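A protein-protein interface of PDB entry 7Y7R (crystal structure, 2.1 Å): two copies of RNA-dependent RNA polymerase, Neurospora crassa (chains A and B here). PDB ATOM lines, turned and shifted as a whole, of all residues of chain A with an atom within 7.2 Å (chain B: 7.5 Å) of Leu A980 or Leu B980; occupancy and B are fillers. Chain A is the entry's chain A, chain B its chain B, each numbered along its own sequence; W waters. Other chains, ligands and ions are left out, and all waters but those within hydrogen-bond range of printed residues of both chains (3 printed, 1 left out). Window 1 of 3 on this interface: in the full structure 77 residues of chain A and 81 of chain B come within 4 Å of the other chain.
The guanidinium group (NH1) of Arg A466 is in hydrogen-bond range of the backbone carbonyl oxygen (O) of Met B976 (2.8 Å).
The backbone carbonyl oxygen of Met A976 lies within hydrogen-bond range of the guanidinium group of Arg B466 (3.0 Å).
The backbone NH of Asp B983 lies within hydrogen-bond range of the backbone carbonyl oxygen of Gly A979, 2.9 Å away.
The backbone NH (N) of Met B981 lies within hydrogen-bond range of the backbone carbonyl oxygen (O) of Met A981.
O of Gly B979 is in hydrogen-bond range of N of Asp A983 (2.8 Å).
NH1 of Arg A466 is in hydrogen-bond range of OD1 of Asn A504 (2.9 Å).
The side-chain hydroxyl (OH) of Tyr A977 is in hydrogen-bond range of the side-chain amide nitrogen (ND2) of Asn A504, 2.8 Å away.
O of Pro B982 sits close to NE2 of Gln B467 (3.4 Å).
OH of Tyr B470 sits close to SD of Met B981 (3.8 Å).
The backbone carbonyl oxygen (O) of Leu B980 is in hydrogen-bond range of the guanidinium group (NH1) of Arg B479.
ND2 of Asn B504 sits at hydrogen-bond distance from OH of Tyr B977, 3.0 Å away.
Among the printed residues, merely in contact across the chains: Arg A466 with Gly B979, Arg A466 with Leu B980, Tyr A470 with Asp B983, Arg A479 with Phe B986, Asn A504 with Met B972, Asn A504 with Met B976, Met A972 with Asn B504, Met A972 with Met B972, Met A972 with Tyr B977, Phe A975 with Phe B986, Met A976 with Asn B504, Tyr A977 with Met B972, Ala A978 with Phe B986, Gly A979 with Arg B466, Gly A979 with Pro B982, Gly A979 with Phe B986, Leu A980 with Arg B466, Leu A980 with Leu B980, Leu A980 with Met B981, Leu A980 with Pro B982, Met A981 with Leu B980, Met A981 with Asp B983, Pro A982 with Gly B979, Pro A982 with Leu B980, Pro A982 with Met B981, Asp A983 with Met B981, Phe A986 with Arg B479, Phe A986 with Phe B975 and Phe A986 with Gly B979.
Leu A980 touches four residues of chain B.
Leu B980 touches just these residues of chain A: Arg A466, Leu A980, Met A981 and Pro A982.
Printed residues of chain B within 4 Å of Arg A466: Met B976 (2.8 Å), Gly B979 (3.5 Å) and Leu B980 (3.2 Å).
Of the printed residues of chain B, Arg A479 touches Phe B986 (3.5 Å).
Printed residues of chain B within 4 Å of Pro A982: Gly B979 (3.7 Å), Leu B980 (3.6 Å) and Met B981 (3.9 Å).
Of the printed residues of chain B, Asn A504 touches Met B972 and Met B976.
The nearest residue of chain B that does not touch Leu A980 is Asp B983 (4.4 Å).
Hydrophobic or aromatic side chains of chain A within 4 Å of the printed part of chain B: Tyr A470, Met A972, Phe A975, Met A976, Tyr A977, Leu A980, Met A981 and Phe A986.
Among the printed residues, no Asp or Glu carboxylate lies within 4 Å of a Lys or Arg side-chain nitrogen of the other chain.
Asn A504 touches Met B976, and with the chains exchanged Met A976 touches Asn B504.
Gly A979 touches Phe B986, and with the chains exchanged Phe A986 touches Gly B979.
Leu A980 touches its own counterpart, Leu B980.
Met B981 touches its own counterpart, Met A981.
16 positions are printed for both chains.
Of the 34 pairs that touch across the chains among the printed residues, 31 have their exchanged pair printed and touching as well.
Water W2 lies within hydrogen-bond range of NH2 of Arg A466 (2.7 Å), O of Phe B975 (2.9 Å) and N of Gly B979 (3.3 Å).
Water W1 lies within hydrogen-bond range of the backbone carbonyl oxygen of Phe A975 (2.7 Å), the guanidinium group of Arg B466 (3.0 Å) and the backbone NH of Gly A979 (3.3 Å).
Water W3 lies within hydrogen-bond range of the backbone carbonyl oxygen of Gly B979 (2.8 Å) and the guanidinium group of Arg A466 (2.8 Å).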
ATOM      1  N   ARG A 466      12.152  30.395 -22.872  1.00  0.00           N
ATOM      2  CA  ARG A 466      12.315  29.364 -23.894  1.00  0.00           C
ATOM      3  C   ARG A 466      10.991  29.078 -24.596  1.00  0.00           C
ATOM      4  O   ARG A 466      10.929  29.048 -25.830  1.00  0.00           O
ATOM      5  CB  ARG A 466      12.888  28.082 -23.273  1.00  0.00           C
ATOM      6  CG  ARG A 466      12.855  26.856 -24.192  1.00  0.00           C
ATOM      7  CD  ARG A 466      13.530  25.622 -23.561  1.00  0.00           C
ATOM      8  NE  ARG A 466      12.716  25.010 -22.516  1.00  0.00           N
ATOM      9  CZ  ARG A 466      13.068  23.948 -21.800  1.00  0.00           C
ATOM     10  NH1 ARG A 466      14.232  23.343 -21.981  1.00  0.00           N
ATOM     11  NH2 ARG A 466      12.230  23.476 -20.884  1.00  0.00           N
ATOM     12  N   GLN A 467       9.917  28.869 -23.821  1.00  0.00           N
ATOM     13  CA  GLN A 467       8.610  28.618 -24.424  1.00  0.00           C
ATOM     14  C   GLN A 467       8.177  29.784 -25.307  1.00  0.00           C
ATOM     15  O   GLN A 467       7.656  29.573 -26.409  1.00  0.00           O
ATOM     16  CB  GLN A 467       7.573  28.337 -23.333  1.00  0.00           C
ATOM     17  CG  GLN A 467       6.253  27.761 -23.846  1.00  0.00           C
ATOM     18  CD  GLN A 467       6.341  26.294 -24.181  1.00  0.00           C
ATOM     19  OE1 GLN A 467       6.821  25.493 -23.380  1.00  0.00           O
ATOM     20  NE2 GLN A 467       5.871  25.927 -25.372  1.00  0.00           N
ATOM     21  N   TYR A 470      10.219  29.798 -28.514  1.00  0.00           N
ATOM     22  CA  TYR A 470       9.783  28.710 -29.386  1.00  0.00           C
ATOM     23  C   TYR A 470       8.481  29.053 -30.098  1.00  0.00           C
ATOM     24  O   TYR A 470       8.307  28.733 -31.280  1.00  0.00           O
ATOM     25  CB  TYR A 470       9.620  27.412 -28.585  1.00  0.00           C
ATOM     26  CG  TYR A 470       9.153  26.253 -29.438  1.00  0.00           C
ATOM     27  CD1 TYR A 470       9.984  25.695 -30.400  1.00  0.00           C
ATOM     28  CD2 TYR A 470       7.872  25.727 -29.294  1.00  0.00           C
ATOM     29  CE1 TYR A 470       9.558  24.640 -31.188  1.00  0.00           C
ATOM     30  CE2 TYR A 470       7.439  24.667 -30.080  1.00  0.00           C
ATOM     31  CZ  TYR A 470       8.285  24.126 -31.023  1.00  0.00           C
ATOM     32  OH  TYR A 470       7.854  23.069 -31.805  1.00  0.00           O
ATOM     33  N   ARG A 479      15.338  22.469 -39.139  1.00  0.00           N
ATOM     34  CA  ARG A 479      15.774  21.293 -38.395  1.00  0.00           C
ATOM     35  C   ARG A 479      15.554  20.013 -39.197  1.00  0.00           C
ATOM     36  O   ARG A 479      16.410  19.117 -39.199  1.00  0.00           O
ATOM     37  CB  ARG A 479      15.029  21.217 -37.062  1.00  0.00           C
ATOM     38  CG  ARG A 479      15.339  22.353 -36.103  1.00  0.00           C
ATOM     39  CD  ARG A 479      14.539  22.209 -34.816  1.00  0.00           C
ATOM     40  NE  ARG A 479      15.113  23.006 -33.742  1.00  0.00           N
ATOM     41  CZ  ARG A 479      15.082  22.666 -32.460  1.00  0.00           C
ATOM     42  NH1 ARG A 479      14.528  21.530 -32.060  1.00  0.00           N
ATOM     43  NH2 ARG A 479      15.620  23.487 -31.558  1.00  0.00           N
ATOM     44  N   ASN A 504      19.237  26.283 -22.485  1.00  0.00           N
ATOM     45  CA  ASN A 504      19.214  24.848 -22.214  1.00  0.00           C
ATOM     46  C   ASN A 504      20.439  24.417 -21.425  1.00  0.00           C
ATOM     47  O   ASN A 504      20.380  23.443 -20.664  1.00  0.00           O
ATOM     48  CB  ASN A 504      19.119  24.057 -23.520  1.00  0.00           C
ATOM     49  CG  ASN A 504      17.703  23.996 -24.063  1.00  0.00           C
ATOM     50  OD1 ASN A 504      16.728  24.080 -23.309  1.00  0.00           O
ATOM     51  ND2 ASN A 504      17.580  23.835 -25.380  1.00  0.00           N
ATOM     52  N   MET A 972      22.969  15.559 -25.277  1.00  0.00           N
ATOM     53  CA  MET A 972      22.232  15.163 -26.466  1.00  0.00           C
ATOM     54  C   MET A 972      23.127  15.167 -27.697  1.00  0.00           C
ATOM     55  O   MET A 972      24.052  15.976 -27.813  1.00  0.00           O
ATOM     56  CB  MET A 972      21.059  16.109 -26.706  1.00  0.00           C
ATOM     57  CG  MET A 972      20.433  16.604 -25.435  1.00  0.00           C
ATOM     58  SD  MET A 972      19.090  15.508 -24.970  1.00  0.00           S
ATOM     59  CE  MET A 972      18.023  15.617 -26.404  1.00  0.00           C
ATOM     60  N   PHE A 975      21.466  15.618 -33.627  1.00  0.00           N
ATOM     61  CA  PHE A 975      20.220  15.223 -34.274  1.00  0.00           C
ATOM     62  C   PHE A 975      19.101  15.018 -33.255  1.00  0.00           C
ATOM     63  O   PHE A 975      17.964  15.457 -33.469  1.00  0.00           O
ATOM     64  CB  PHE A 975      20.436  13.954 -35.102  1.00  0.00           C
ATOM     65  CG  PHE A 975      19.163  13.230 -35.424  1.00  0.00           C
ATOM     66  CD1 PHE A 975      18.249  13.772 -36.319  1.00  0.00           C
ATOM     67  CD2 PHE A 975      18.864  12.029 -34.814  1.00  0.00           C
ATOM     68  CE1 PHE A 975      17.071  13.121 -36.608  1.00  0.00           C
ATOM     69  CE2 PHE A 975      17.685  11.369 -35.104  1.00  0.00           C
ATOM     70  CZ  PHE A 975      16.788  11.916 -35.999  1.00  0.00           C
ATOM     71  N   MET A 976      19.392  14.316 -32.153  1.00  0.00           N
ATOM     72  CA  MET A 976      18.362  14.084 -31.144  1.00  0.00           C
ATOM     73  C   MET A 976      17.879  15.389 -30.529  1.00  0.00           C
ATOM     74  O   MET A 976      16.690  15.532 -30.214  1.00  0.00           O
ATOM     75  CB  MET A 976      18.891  13.132 -30.074  1.00  0.00           C
ATOM     76  CG  MET A 976      19.083  11.725 -30.589  1.00  0.00           C
ATOM     77  SD  MET A 976      17.648  11.144 -31.538  1.00  0.00           S
ATOM     78  CE  MET A 976      16.611  10.406 -30.276  1.00  0.00           C
ATOM     79  N   TYR A 977      18.788  16.352 -30.355  1.00  0.00           N
ATOM     80  CA  TYR A 977      18.410  17.657 -29.819  1.00  0.00           C
ATOM     81  C   TYR A 977      17.403  18.359 -30.723  1.00  0.00           C
ATOM     82  O   TYR A 977      16.496  19.049 -30.241  1.00  0.00           O
ATOM     83  CB  TYR A 977      19.662  18.518 -29.643  1.00  0.00           C
ATOM     84  CG  TYR A 977      19.416  19.932 -29.180  1.00  0.00           C
ATOM     85  CD1 TYR A 977      19.226  20.217 -27.835  1.00  0.00           C
ATOM     86  CD2 TYR A 977      19.397  20.989 -30.083  1.00  0.00           C
ATOM     87  CE1 TYR A 977      19.007  21.514 -27.405  1.00  0.00           C
ATOM     88  CE2 TYR A 977      19.182  22.291 -29.662  1.00  0.00           C
ATOM     89  CZ  TYR A 977      18.989  22.551 -28.323  1.00  0.00           C
ATOM     90  OH  TYR A 977      18.780  23.854 -27.898  1.00  0.00           O
ATOM     91  N   ALA A 978      17.551  18.205 -32.040  1.00  0.00           N
ATOM     92  CA  ALA A 978      16.709  18.961 -32.962  1.00  0.00           C
ATOM     93  C   ALA A 978      15.286  18.424 -33.029  1.00  0.00           C
ATOM     94  O   ALA A 978      14.378  19.158 -33.432  1.00  0.00           O
ATOM     95  CB  ALA A 978      17.337  18.972 -34.355  1.00  0.00           C
ATOM     96  N   GLY A 979      15.071  17.167 -32.649  1.00  0.00           N
ATOM     97  CA  GLY A 979      13.754  16.569 -32.638  1.00  0.00           C
ATOM     98  C   GLY A 979      12.908  16.871 -31.422  1.00  0.00           C
ATOM     99  O   GLY A 979      11.755  16.437 -31.373  1.00  0.00           O
ATOM    100  N   LEU A 980      13.437  17.600 -30.442  1.00  0.00           N
ATOM    101  CA  LEU A 980      12.731  17.919 -29.208  1.00  0.00           C
ATOM    102  C   LEU A 980      12.139  19.321 -29.270  1.00  0.00           C
ATOM    103  O   LEU A 980      12.627  20.196 -29.991  1.00  0.00           O
ATOM    104  CB  LEU A 980      13.673  17.812 -28.004  1.00  0.00           C
ATOM    105  CG  LEU A 980      14.187  16.430 -27.593  1.00  0.00           C
ATOM    106  CD1 LEU A 980      14.744  16.487 -26.189  1.00  0.00           C
ATOM    107  CD2 LEU A 980      13.083  15.382 -27.678  1.00  0.00           C
ATOM    108  N   MET A 981      11.087  19.534 -28.487  1.00  0.00           N
ATOM    109  CA  MET A 981      10.443  20.837 -28.392  1.00  0.00           C
ATOM    110  C   MET A 981       9.964  21.073 -26.967  1.00  0.00           C
ATOM    111  O   MET A 981       9.625  20.118 -26.255  1.00  0.00           O
ATOM    112  CB  MET A 981       9.257  20.959 -29.365  1.00  0.00           C
ATOM    113  CG  MET A 981       8.272  19.787 -29.300  1.00  0.00           C
ATOM    114  SD  MET A 981       6.534  20.207 -29.612  1.00  0.00           S
ATOM    115  CE  MET A 981       6.520  20.351 -31.394  1.00  0.00           C
ATOM    116  N   PRO A 982       9.917  22.333 -26.530  1.00  0.00           N
ATOM    117  CA  PRO A 982       9.412  22.635 -25.185  1.00  0.00           C
ATOM    118  C   PRO A 982       8.026  22.059 -24.951  1.00  0.00           C
ATOM    119  O   PRO A 982       7.197  21.977 -25.859  1.00  0.00           O
ATOM    120  CB  PRO A 982       9.383  24.167 -25.153  1.00  0.00           C
ATOM    121  CG  PRO A 982      10.402  24.584 -26.157  1.00  0.00           C
ATOM    122  CD  PRO A 982      10.334  23.546 -27.251  1.00  0.00           C
ATOM    123  N   ASP A 983       7.783  21.659 -23.707  1.00  0.00           N
ATOM    124  CA  ASP A 983       6.508  21.087 -23.284  1.00  0.00           C
ATOM    125  C   ASP A 983       5.718  22.191 -22.594  1.00  0.00           C
ATOM    126  O   ASP A 983       5.935  22.474 -21.412  1.00  0.00           O
ATOM    127  CB  ASP A 983       6.732  19.897 -22.357  1.00  0.00           C
ATOM    128  CG  ASP A 983       5.430  19.257 -21.891  1.00  0.00           C
ATOM    129  OD1 ASP A 983       4.342  19.837 -22.117  1.00  0.00           O
ATOM    130  OD2 ASP A 983       5.498  18.155 -21.306  1.00  0.00           O
ATOM    131  N   PHE A 986       4.281  21.284 -19.431  1.00  0.00           N
ATOM    132  CA  PHE A 986       5.266  21.237 -18.318  1.00  0.00           C
ATOM    133  C   PHE A 986       5.519  22.649 -17.803  1.00  0.00           C
ATOM    134  O   PHE A 986       5.592  22.824 -16.584  1.00  0.00           O
ATOM    135  CB  PHE A 986       6.594  20.613 -18.757  1.00  0.00           C
ATOM    136  CG  PHE A 986       7.722  20.704 -17.758  1.00  0.00           C
ATOM    137  CD1 PHE A 986       8.544  21.817 -17.703  1.00  0.00           C
ATOM    138  CD2 PHE A 986       7.977  19.661 -16.884  1.00  0.00           C
ATOM    139  CE1 PHE A 986       9.575  21.898 -16.783  1.00  0.00           C
ATOM    140  CE2 PHE A 986       9.011  19.741 -15.966  1.00  0.00           C
ATOM    141  CZ  PHE A 986       9.811  20.857 -15.919  1.00  0.00           C
ATOM    142  N   ARG B 466      11.593   6.952 -29.896  1.00  0.00           N
ATOM    143  CA  ARG B 466      11.454   7.953 -28.852  1.00  0.00           C
ATOM    144  C   ARG B 466      10.021   8.463 -28.801  1.00  0.00           C
ATOM    145  O   ARG B 466       9.419   8.544 -27.722  1.00  0.00           O
ATOM    146  CB  ARG B 466      12.437   9.098 -29.075  1.00  0.00           C
ATOM    147  CG  ARG B 466      12.399  10.122 -27.969  1.00  0.00           C
ATOM    148  CD  ARG B 466      13.423  11.199 -28.182  1.00  0.00           C
ATOM    149  NE  ARG B 466      13.293  11.872 -29.465  1.00  0.00           N
ATOM    150  CZ  ARG B 466      14.124  12.821 -29.873  1.00  0.00           C
ATOM    151  NH1 ARG B 466      15.139  13.213 -29.121  1.00  0.00           N
ATOM    152  NH2 ARG B 466      13.931  13.393 -31.061  1.00  0.00           N
ATOM    153  N   GLN B 467       9.449   8.783 -29.967  1.00  0.00           N
ATOM    154  CA  GLN B 467       8.073   9.273 -30.012  1.00  0.00           C
ATOM    155  C   GLN B 467       7.093   8.246 -29.461  1.00  0.00           C
ATOM    156  O   GLN B 467       6.209   8.588 -28.670  1.00  0.00           O
ATOM    157  CB  GLN B 467       7.691   9.651 -31.440  1.00  0.00           C
ATOM    158  CG  GLN B 467       6.729  10.816 -31.514  1.00  0.00           C
ATOM    159  CD  GLN B 467       7.446  12.104 -31.799  1.00  0.00           C
ATOM    160  OE1 GLN B 467       8.393  12.129 -32.577  1.00  0.00           O
ATOM    161  NE2 GLN B 467       6.999  13.187 -31.180  1.00  0.00           N
ATOM    162  N   TYR B 470       7.472   7.934 -25.739  1.00  0.00           N
ATOM    163  CA  TYR B 470       6.891   9.089 -25.069  1.00  0.00           C
ATOM    164  C   TYR B 470       5.374   8.980 -24.985  1.00  0.00           C
ATOM    165  O   TYR B 470       4.773   9.378 -23.981  1.00  0.00           O
ATOM    166  CB  TYR B 470       7.289  10.372 -25.794  1.00  0.00           C
ATOM    167  CG  TYR B 470       6.482  11.576 -25.362  1.00  0.00           C
ATOM    168  CD1 TYR B 470       6.753  12.220 -24.161  1.00  0.00           C
ATOM    169  CD2 TYR B 470       5.441  12.058 -26.144  1.00  0.00           C
ATOM    170  CE1 TYR B 470       6.019  13.320 -23.755  1.00  0.00           C
ATOM    171  CE2 TYR B 470       4.698  13.158 -25.743  1.00  0.00           C
ATOM    172  CZ  TYR B 470       4.992  13.786 -24.546  1.00  0.00           C
ATOM    173  OH  TYR B 470       4.260  14.881 -24.138  1.00  0.00           O
ATOM    174  N   ARG B 479       8.047  14.611 -13.736  1.00  0.00           N
ATOM    175  CA  ARG B 479       9.031  15.645 -14.035  1.00  0.00           C
ATOM    176  C   ARG B 479       8.680  16.967 -13.361  1.00  0.00           C
ATOM    177  O   ARG B 479       9.572  17.670 -12.866  1.00  0.00           O
ATOM    178  CB  ARG B 479       9.155  15.829 -15.547  1.00  0.00           C
ATOM    179  CG  ARG B 479       9.778  14.647 -16.257  1.00  0.00           C
ATOM    180  CD  ARG B 479       9.610  14.755 -17.764  1.00  0.00           C
ATOM    181  NE  ARG B 479      10.509  13.848 -18.465  1.00  0.00           N
ATOM    182  CZ  ARG B 479      11.181  14.147 -19.570  1.00  0.00           C
ATOM    183  NH1 ARG B 479      11.090  15.342 -20.135  1.00  0.00           N
ATOM    184  NH2 ARG B 479      11.966  13.222 -20.120  1.00  0.00           N
ATOM    185  N   ASN B 500      14.595   6.754 -23.441  1.00  0.00           N
ATOM    186  CA  ASN B 500      14.688   8.058 -24.085  1.00  0.00           C
ATOM    187  C   ASN B 500      16.004   8.744 -23.739  1.00  0.00           C
ATOM    188  O   ASN B 500      16.699   9.262 -24.622  1.00  0.00           O
ATOM    189  CB  ASN B 500      13.492   8.922 -23.694  1.00  0.00           C
ATOM    190  CG  ASN B 500      12.236   8.545 -24.471  1.00  0.00           C
ATOM    191  OD1 ASN B 500      12.254   7.603 -25.265  1.00  0.00           O
ATOM    192  ND2 ASN B 500      11.161   9.307 -24.288  1.00  0.00           N
ATOM    193  N   ASN B 504      18.623   9.641 -26.572  1.00  0.00           N
ATOM    194  CA  ASN B 504      19.027  11.019 -26.809  1.00  0.00           C
ATOM    195  C   ASN B 504      20.531  11.163 -26.878  1.00  0.00           C
ATOM    196  O   ASN B 504      21.023  12.133 -27.456  1.00  0.00           O
ATOM    197  CB  ASN B 504      18.469  11.928 -25.719  1.00  0.00           C
ATOM    198  CG  ASN B 504      17.017  12.219 -25.926  1.00  0.00           C
ATOM    199  OD1 ASN B 504      16.521  12.155 -27.048  1.00  0.00           O
ATOM    200  ND2 ASN B 504      16.314  12.522 -24.851  1.00  0.00           N
ATOM    201  N   MET B 972      22.390  19.637 -21.960  1.00  0.00           N
ATOM    202  CA  MET B 972      21.236  20.170 -21.232  1.00  0.00           C
ATOM    203  C   MET B 972      21.420  20.021 -19.727  1.00  0.00           C
ATOM    204  O   MET B 972      21.851  18.964 -19.251  1.00  0.00           O
ATOM    205  CB  MET B 972      19.961  19.411 -21.590  1.00  0.00           C
ATOM    206  CG  MET B 972      19.822  18.974 -23.017  1.00  0.00           C
ATOM    207  SD  MET B 972      18.925  20.131 -24.010  1.00  0.00           S
ATOM    208  CE  MET B 972      17.520  20.425 -22.946  1.00  0.00           C
ATOM    209  N   PHE B 975      17.189  20.218 -15.245  1.00  0.00           N
ATOM    210  CA  PHE B 975      15.892  20.886 -15.277  1.00  0.00           C
ATOM    211  C   PHE B 975      15.440  21.153 -16.711  1.00  0.00           C
ATOM    212  O   PHE B 975      14.333  20.765 -17.108  1.00  0.00           O
ATOM    213  CB  PHE B 975      15.940  22.188 -14.475  1.00  0.00           C
ATOM    214  CG  PHE B 975      14.724  23.034 -14.655  1.00  0.00           C
ATOM    215  CD1 PHE B 975      13.480  22.563 -14.261  1.00  0.00           C
ATOM    216  CD2 PHE B 975      14.810  24.279 -15.254  1.00  0.00           C
ATOM    217  CE1 PHE B 975      12.348  23.332 -14.438  1.00  0.00           C
ATOM    218  CE2 PHE B 975      13.686  25.050 -15.429  1.00  0.00           C
ATOM    219  CZ  PHE B 975      12.450  24.576 -15.021  1.00  0.00           C
ATOM    220  N   MET B 976      16.290  21.813 -17.507  1.00  0.00           N
ATOM    221  CA  MET B 976      15.896  22.160 -18.869  1.00  0.00           C
ATOM    222  C   MET B 976      15.652  20.919 -19.720  1.00  0.00           C
ATOM    223  O   MET B 976      14.773  20.927 -20.590  1.00  0.00           O
ATOM    224  CB  MET B 976      16.944  23.090 -19.493  1.00  0.00           C
ATOM    225  CG  MET B 976      17.068  24.395 -18.731  1.00  0.00           C
ATOM    226  SD  MET B 976      15.529  25.372 -18.680  1.00  0.00           S
ATOM    227  CE  MET B 976      15.374  25.974 -20.361  1.00  0.00           C
ATOM    228  N   TYR B 977      16.383  19.831 -19.468  1.00  0.00           N
ATOM    229  CA  TYR B 977      16.085  18.594 -20.181  1.00  0.00           C
ATOM    230  C   TYR B 977      14.665  18.113 -19.887  1.00  0.00           C
ATOM    231  O   TYR B 977      13.967  17.635 -20.788  1.00  0.00           O
ATOM    232  CB  TYR B 977      17.113  17.522 -19.818  1.00  0.00           C
ATOM    233  CG  TYR B 977      16.807  16.148 -20.361  1.00  0.00           C
ATOM    234  CD1 TYR B 977      17.102  15.818 -21.678  1.00  0.00           C
ATOM    235  CD2 TYR B 977      16.244  15.170 -19.549  1.00  0.00           C
ATOM    236  CE1 TYR B 977      16.829  14.548 -22.178  1.00  0.00           C
ATOM    237  CE2 TYR B 977      15.974  13.905 -20.034  1.00  0.00           C
ATOM    238  CZ  TYR B 977      16.268  13.595 -21.348  1.00  0.00           C
ATOM    239  OH  TYR B 977      15.993  12.329 -21.830  1.00  0.00           O
ATOM    240  N   ALA B 978      14.203  18.261 -18.637  1.00  0.00           N
ATOM    241  CA  ALA B 978      12.911  17.682 -18.255  1.00  0.00           C
ATOM    242  C   ALA B 978      11.733  18.387 -18.921  1.00  0.00           C
ATOM    243  O   ALA B 978      10.687  17.765 -19.154  1.00  0.00           O
ATOM    244  CB  ALA B 978      12.740  17.719 -16.739  1.00  0.00           C
ATOM    245  N   GLY B 979      11.870  19.670 -19.218  1.00  0.00           N
ATOM    246  CA  GLY B 979      10.799  20.420 -19.825  1.00  0.00           C
ATOM    247  C   GLY B 979      10.646  20.264 -21.320  1.00  0.00           C
ATOM    248  O   GLY B 979       9.763  20.902 -21.893  1.00  0.00           O
ATOM    249  N   LEU B 980      11.465  19.444 -21.977  1.00  0.00           N
ATOM    250  CA  LEU B 980      11.355  19.214 -23.412  1.00  0.00           C
ATOM    251  C   LEU B 980      10.584  17.927 -23.685  1.00  0.00           C
ATOM    252  O   LEU B 980      10.556  17.017 -22.855  1.00  0.00           O
ATOM    253  CB  LEU B 980      12.744  19.136 -24.050  1.00  0.00           C
ATOM    254  CG  LEU B 980      13.587  20.411 -23.995  1.00  0.00           C
ATOM    255  CD1 LEU B 980      14.700  20.378 -25.024  1.00  0.00           C
ATOM    256  CD2 LEU B 980      12.703  21.617 -24.222  1.00  0.00           C
ATOM    257  N   MET B 981       9.969  17.848 -24.857  1.00  0.00           N
ATOM    258  CA  MET B 981       9.247  16.660 -25.286  1.00  0.00           C
ATOM    259  C   MET B 981       9.515  16.401 -26.763  1.00  0.00           C
ATOM    260  O   MET B 981       9.951  17.300 -27.488  1.00  0.00           O
ATOM    261  CB  MET B 981       7.737  16.798 -25.051  1.00  0.00           C
ATOM    262  CG  MET B 981       7.134  18.079 -25.621  1.00  0.00           C
ATOM    263  SD  MET B 981       5.406  17.921 -26.108  1.00  0.00           S
ATOM    264  CE  MET B 981       4.612  17.906 -24.506  1.00  0.00           C
ATOM    265  N   PRO B 982       9.270  15.177 -27.226  1.00  0.00           N
ATOM    266  CA  PRO B 982       9.482  14.886 -28.650  1.00  0.00           C
ATOM    267  C   PRO B 982       8.509  15.664 -29.524  1.00  0.00           C
ATOM    268  O   PRO B 982       7.347  15.873 -29.164  1.00  0.00           O
ATOM    269  CB  PRO B 982       9.243  13.373 -28.743  1.00  0.00           C
ATOM    270  CG  PRO B 982       9.431  12.866 -27.334  1.00  0.00           C
ATOM    271  CD  PRO B 982       8.903  13.973 -26.467  1.00  0.00           C
ATOM    272  N   ASP B 983       9.009  16.108 -30.676  1.00  0.00           N
ATOM    273  CA  ASP B 983       8.236  16.884 -31.643  1.00  0.00           C
ATOM    274  C   ASP B 983       7.626  15.917 -32.652  1.00  0.00           C
ATOM    275  O   ASP B 983       8.331  15.400 -33.527  1.00  0.00           O
ATOM    276  CB  ASP B 983       9.129  17.925 -32.322  1.00  0.00           C
ATOM    277  CG  ASP B 983       8.371  18.819 -33.293  1.00  0.00           C
ATOM    278  OD1 ASP B 983       7.230  18.468 -33.662  1.00  0.00           O
ATOM    279  OD2 ASP B 983       8.907  19.890 -33.667  1.00  0.00           O
ATOM    280  N   PHE B 986       8.297  16.823 -36.327  1.00  0.00           N
ATOM    281  CA  PHE B 986       9.661  16.553 -36.770  1.00  0.00           C
ATOM    282  C   PHE B 986       9.833  15.082 -37.149  1.00  0.00           C
ATOM    283  O   PHE B 986      10.397  14.762 -38.204  1.00  0.00           O
ATOM    284  CB  PHE B 986      10.648  16.975 -35.675  1.00  0.00           C
ATOM    285  CG  PHE B 986      12.084  16.751 -36.033  1.00  0.00           C
ATOM    286  CD1 PHE B 986      12.806  17.725 -36.699  1.00  0.00           C
ATOM    287  CD2 PHE B 986      12.720  15.571 -35.689  1.00  0.00           C
ATOM    288  CE1 PHE B 986      14.133  17.521 -37.033  1.00  0.00           C
ATOM    289  CE2 PHE B 986      14.049  15.361 -36.018  1.00  0.00           C
ATOM    290  CZ  PHE B 986      14.754  16.335 -36.691  1.00  0.00           C
HETATM  291  O   HOH W   1      15.632  14.003 -33.463  1.00  0.00           O
HETATM  292  O   HOH W   2      12.617  22.784 -18.287  1.00  0.00           O
HETATM  293  O   HOH W   3       9.427  23.481 -20.936  1.00  0.00           O
